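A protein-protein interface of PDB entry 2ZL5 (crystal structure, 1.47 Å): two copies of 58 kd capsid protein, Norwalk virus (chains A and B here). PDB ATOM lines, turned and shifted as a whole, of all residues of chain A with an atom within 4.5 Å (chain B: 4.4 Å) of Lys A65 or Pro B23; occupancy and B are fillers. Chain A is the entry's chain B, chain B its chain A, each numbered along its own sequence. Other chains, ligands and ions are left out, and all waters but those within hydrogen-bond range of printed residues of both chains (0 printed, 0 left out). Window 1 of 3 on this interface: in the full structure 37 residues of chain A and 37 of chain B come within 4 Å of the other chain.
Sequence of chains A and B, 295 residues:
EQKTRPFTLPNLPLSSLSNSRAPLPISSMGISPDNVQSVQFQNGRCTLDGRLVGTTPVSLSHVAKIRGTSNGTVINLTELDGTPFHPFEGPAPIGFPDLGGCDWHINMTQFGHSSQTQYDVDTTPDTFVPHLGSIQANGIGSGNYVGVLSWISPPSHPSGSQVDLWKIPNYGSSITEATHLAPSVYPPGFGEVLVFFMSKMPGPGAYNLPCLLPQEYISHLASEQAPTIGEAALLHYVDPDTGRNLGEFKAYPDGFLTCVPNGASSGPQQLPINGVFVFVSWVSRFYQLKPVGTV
O of Pro B23 is in hydrogen-bond range of NZ of Lys A65 (2.8 Å).
The backbone NH (N) of Lys A65 lies within hydrogen-bond range of the backbone carbonyl oxygen (O) of Gly A95, at 3.1 Å. The side-chain hydroxyl of Ser B18 lies within hydrogen-bond range of the backbone carbonyl oxygen of Leu B24, 3.4 Å away. O of Ser A61 sits at hydrogen-bond distance from NZ of Lys A65 (2.8 Å). The side-chain hydroxyl (OG) of Ser A61 sits at hydrogen-bond distance from a ring nitrogen (ND1) of His A62, 3.2 Å away.
Among the printed residues, pairs that only touch across the chains: Ser A61 with Ser B18, Ser A61 with Leu B60, Ser A61 with Leu B24 and Ser A61 with Pro B23.
Printed residues of chain B within 4 Å of Ser A61: Ser B18 (3.4 Å), Pro B23 (3.9 Å), Leu B24 (3.8 Å) and Leu B60 (3.4 Å). Lys A65 touches just one residue of chain B: Pro B23. Of the printed residues of chain A, Ser B18 touches Ser A61. Pro B23 touches just these residues of chain A: Ser A61 and Lys A65. Printed residues of chain A within 4 Å of Leu B60: Ser A61 (3.4 Å). The nearest printed residue of chain B that does not touch Lys A65 is Leu B24 (4.8 Å). The nearest printed residue of chain B that does not touch Ser A61 is Ala B22 (5.9 Å).
Printed residues of chain A that touch a printed residue of chain B: Ser A61 and Lys A65. Of the 6 printed residues of chain B, 4 touch a printed residue of chain A. Printed residues of chain B that touch a printed residue of chain A: Ser B18, Pro B23, Leu B24 and Leu B60. Hydrophobic or aromatic side chains of chain B that line the printed part of chain A: Leu B60. Among the printed residues, 5 pairs touch across the chains.
Position printed for both chains: 63. Of the 5 pairs that touch across the chains among the printed residues, none has its exchanged pair printed and touching as well.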
ATOM      1  N   SER A  61      15.364  20.308  16.510  1.00  0.00           N
ATOM      2  CA  SER A  61      14.805  18.948  16.400  1.00  0.00           C
ATOM      3  C   SER A  61      15.550  18.070  15.416  1.00  0.00           C
ATOM      4  O   SER A  61      15.340  16.867  15.420  1.00  0.00           O
ATOM      5  CB  SER A  61      13.324  18.971  16.037  1.00  0.00           C
ATOM      6  OG  SER A  61      13.075  19.610  14.797  1.00  0.00           O
ATOM      7  N   HIS A  62      16.399  18.674  14.575  1.00  0.00           N
ATOM      8  CA  HIS A  62      17.221  17.930  13.623  1.00  0.00           C
ATOM      9  C   HIS A  62      18.694  17.821  14.037  1.00  0.00           C
ATOM     10  O   HIS A  62      19.471  17.174  13.360  1.00  0.00           O
ATOM     11  CB  HIS A  62      17.209  18.617  12.260  1.00  0.00           C
ATOM     12  CG  HIS A  62      15.893  18.626  11.541  1.00  0.00           C
ATOM     13  ND1 HIS A  62      14.693  19.042  12.082  1.00  0.00           N
ATOM     14  CD2 HIS A  62      15.642  18.365  10.232  1.00  0.00           C
ATOM     15  CE1 HIS A  62      13.745  18.982  11.146  1.00  0.00           C
ATOM     16  NE2 HIS A  62      14.304  18.573  10.019  1.00  0.00           N
ATOM     17  N   VAL A  63      19.093  18.493  15.119  1.00  0.00           N
ATOM     18  CA  VAL A  63      20.516  18.635  15.439  1.00  0.00           C
ATOM     19  C   VAL A  63      21.099  17.402  16.133  1.00  0.00           C
ATOM     20  O   VAL A  63      20.554  16.907  17.132  1.00  0.00           O
ATOM     21  CB  VAL A  63      20.756  19.883  16.330  1.00  0.00           C
ATOM     22  CG1 VAL A  63      22.162  19.880  16.923  1.00  0.00           C
ATOM     23  CG2 VAL A  63      20.591  21.147  15.496  1.00  0.00           C
ATOM     24  N   ALA A  64      22.214  16.917  15.574  1.00  0.00           N
ATOM     25  CA  ALA A  64      22.931  15.734  16.091  1.00  0.00           C
ATOM     26  C   ALA A  64      22.068  14.469  16.041  1.00  0.00           C
ATOM     27  O   ALA A  64      22.039  13.670  16.974  1.00  0.00           O
ATOM     28  CB  ALA A  64      23.476  15.971  17.509  1.00  0.00           C
ATOM     29  N   LYS A  65      21.345  14.339  14.921  1.00  0.00           N
ATOM     30  CA  LYS A  65      20.484  13.192  14.696  1.00  0.00           C
ATOM     31  C   LYS A  65      20.881  12.454  13.439  1.00  0.00           C
ATOM     32  O   LYS A  65      21.540  13.009  12.559  1.00  0.00           O
ATOM     33  CB  LYS A  65      19.017  13.593  14.621  1.00  0.00           C
ATOM     34  CG  LYS A  65      18.456  14.031  15.990  1.00  0.00           C
ATOM     35  CD  LYS A  65      16.956  14.091  15.980  1.00  0.00           C
ATOM     36  CE  LYS A  65      16.417  14.551  17.319  1.00  0.00           C
ATOM     37  NZ  LYS A  65      14.925  14.690  17.189  1.00  0.00           N
ATOM     38  N   ILE A  66      20.526  11.162  13.426  1.00  0.00           N
ATOM     39  CA  ILE A  66      20.714  10.318  12.234  1.00  0.00           C
ATOM     40  C   ILE A  66      19.401   9.600  11.922  1.00  0.00           C
ATOM     41  O   ILE A  66      18.578   9.389  12.796  1.00  0.00           O
ATOM     42  CB  ILE A  66      21.861   9.294  12.403  1.00  0.00           C
ATOM     43  CG1 ILE A  66      21.511   8.188  13.405  1.00  0.00           C
ATOM     44  CG2 ILE A  66      23.158  10.013  12.757  1.00  0.00           C
ATOM     45  CD1 ILE A  66      22.534   7.046  13.359  1.00  0.00           C
ATOM     46  N   LEU A  80      16.456  13.088   7.791  1.00  0.00           N
ATOM     47  CA  LEU A  80      15.671  12.730   8.962  1.00  0.00           C
ATOM     48  C   LEU A  80      14.248  12.333   8.629  1.00  0.00           C
ATOM     49  O   LEU A  80      13.678  11.475   9.305  1.00  0.00           O
ATOM     50  CB  LEU A  80      15.668  13.862   9.979  1.00  0.00           C
ATOM     51  CG  LEU A  80      16.990  14.090  10.688  1.00  0.00           C
ATOM     52  CD1 LEU A  80      16.636  14.921  11.914  1.00  0.00           C
ATOM     53  CD2 LEU A  80      17.690  12.787  11.075  1.00  0.00           C
ATOM     54  N   GLY A  95      21.835  17.840   9.761  1.00  0.00           N
ATOM     55  CA  GLY A  95      21.759  17.572  11.194  1.00  0.00           C
ATOM     56  C   GLY A  95      22.695  16.496  11.719  1.00  0.00           C
ATOM     57  O   GLY A  95      22.788  16.283  12.934  1.00  0.00           O
ATOM     58  N   PHE A  96      23.380  15.777  10.823  1.00  0.00           N
ATOM     59  CA  PHE A  96      24.209  14.645  11.266  1.00  0.00           C
ATOM     60  C   PHE A  96      25.229  15.185  12.289  1.00  0.00           C
ATOM     61  O   PHE A  96      25.733  16.281  12.114  1.00  0.00           O
ATOM     62  CB  PHE A  96      24.940  14.092  10.023  1.00  0.00           C
ATOM     63  CG  PHE A  96      25.631  12.775  10.238  1.00  0.00           C
ATOM     64  CD1 PHE A  96      24.928  11.565  10.070  1.00  0.00           C
ATOM     65  CD2 PHE A  96      26.995  12.726  10.545  1.00  0.00           C
ATOM     66  CE1 PHE A  96      25.585  10.334  10.275  1.00  0.00           C
ATOM     67  CE2 PHE A  96      27.638  11.483  10.751  1.00  0.00           C
ATOM     68  CZ  PHE A  96      26.913  10.299  10.610  1.00  0.00           C
ATOM     69  N   PRO A  97      25.559  14.403  13.334  1.00  0.00           N
ATOM     70  CA  PRO A  97      26.536  14.968  14.301  1.00  0.00           C
ATOM     71  C   PRO A  97      27.866  15.354  13.680  1.00  0.00           C
ATOM     72  O   PRO A  97      28.347  14.671  12.770  1.00  0.00           O
ATOM     73  CB  PRO A  97      26.718  13.841  15.323  1.00  0.00           C
ATOM     74  CG  PRO A  97      25.452  13.018  15.204  1.00  0.00           C
ATOM     75  CD  PRO A  97      25.104  13.055  13.736  1.00  0.00           C
ATOM     76  N   GLY A 147      18.101   8.217  15.327  1.00  0.00           N
ATOM     77  CA  GLY A 147      19.060   8.268  16.446  1.00  0.00           C
ATOM     78  C   GLY A 147      19.362   9.700  16.822  1.00  0.00           C
ATOM     79  O   GLY A 147      19.394  10.583  15.963  1.00  0.00           O
ATOM     80  N   VAL A 148      19.602   9.921  18.118  1.00  0.00           N
ATOM     81  CA  VAL A 148      20.040  11.255  18.586  1.00  0.00           C
ATOM     82  C   VAL A 148      21.266  11.049  19.466  1.00  0.00           C
ATOM     83  O   VAL A 148      21.299  10.128  20.280  1.00  0.00           O
ATOM     84  CB  VAL A 148      18.921  12.004  19.361  1.00  0.00           C
ATOM     85  CG1 VAL A 148      18.411  11.217  20.571  1.00  0.00           C
ATOM     86  CG2 VAL A 148      19.378  13.430  19.724  1.00  0.00           C
ATOM     87  N   SER B  18       9.961  22.495  14.857  1.00  0.00           N
ATOM     88  CA  SER B  18       9.804  21.444  15.863  1.00  0.00           C
ATOM     89  C   SER B  18       8.492  21.520  16.634  1.00  0.00           C
ATOM     90  O   SER B  18       7.950  22.596  16.848  1.00  0.00           O
ATOM     91  CB  SER B  18      10.907  21.576  16.943  1.00  0.00           C
ATOM     92  OG  SER B  18      10.867  20.507  17.876  1.00  0.00           O
ATOM     93  N   ALA B  22       7.822  17.848  22.444  1.00  0.00           N
ATOM     94  CA  ALA B  22       8.934  16.896  22.354  1.00  0.00           C
ATOM     95  C   ALA B  22       9.830  17.351  21.196  1.00  0.00           C
ATOM     96  O   ALA B  22       9.353  18.056  20.320  1.00  0.00           O
ATOM     97  CB  ALA B  22       8.428  15.459  22.145  1.00  0.00           C
ATOM     98  N   PRO B  23      11.120  16.998  21.239  1.00  0.00           N
ATOM     99  CA  PRO B  23      12.046  17.497  20.188  1.00  0.00           C
ATOM    100  C   PRO B  23      11.897  16.719  18.860  1.00  0.00           C
ATOM    101  O   PRO B  23      12.807  15.961  18.446  1.00  0.00           O
ATOM    102  CB  PRO B  23      13.419  17.291  20.829  1.00  0.00           C
ATOM    103  CG  PRO B  23      13.226  16.093  21.720  1.00  0.00           C
ATOM    104  CD  PRO B  23      11.823  16.238  22.303  1.00  0.00           C
ATOM    105  N   LEU B  24      10.756  16.928  18.201  1.00  0.00           N
ATOM    106  CA  LEU B  24      10.397  16.167  16.982  1.00  0.00           C
ATOM    107  C   LEU B  24      10.017  17.107  15.858  1.00  0.00           C
ATOM    108  O   LEU B  24       9.314  18.095  16.075  1.00  0.00           O
ATOM    109  CB  LEU B  24       9.175  15.268  17.229  1.00  0.00           C
ATOM    110  CG  LEU B  24       9.277  14.226  18.340  1.00  0.00           C
ATOM    111  CD1 LEU B  24       7.892  13.700  18.652  1.00  0.00           C
ATOM    112  CD2 LEU B  24      10.253  13.095  18.015  1.00  0.00           C
ATOM    113  N   LEU B  60      14.135  24.541  22.683  1.00  0.00           N
ATOM    114  CA  LEU B  60      13.867  23.114  22.577  1.00  0.00           C
ATOM    115  C   LEU B  60      14.837  22.252  23.397  1.00  0.00           C
ATOM    116  O   LEU B  60      14.523  21.108  23.732  1.00  0.00           O
ATOM    117  CB  LEU B  60      13.916  22.677  21.099  1.00  0.00           C
ATOM    118  CG  LEU B  60      13.262  21.319  20.839  1.00  0.00           C
ATOM    119  CD1 LEU B  60      11.736  21.445  20.898  1.00  0.00           C
ATOM    120  CD2 LEU B  60      13.701  20.882  19.458  1.00  0.00           C
ATOM    121  N   VAL B  63      13.001  20.995  26.317  1.00  0.00           N
ATOM    122  CA  VAL B  63      11.659  20.429  26.145  1.00  0.00           C
ATOM    123  C   VAL B  63      11.613  18.920  26.380  1.00  0.00           C
ATOM    124  O   VAL B  63      12.377  18.172  25.808  1.00  0.00           O
ATOM    125  CB  VAL B  63      11.094  20.784  24.738  1.00  0.00           C
ATOM    126  CG1 VAL B  63       9.825  19.956  24.416  1.00  0.00           C
ATOM    127  CG2 VAL B  63      10.780  22.260  24.671  1.00  0.00           C
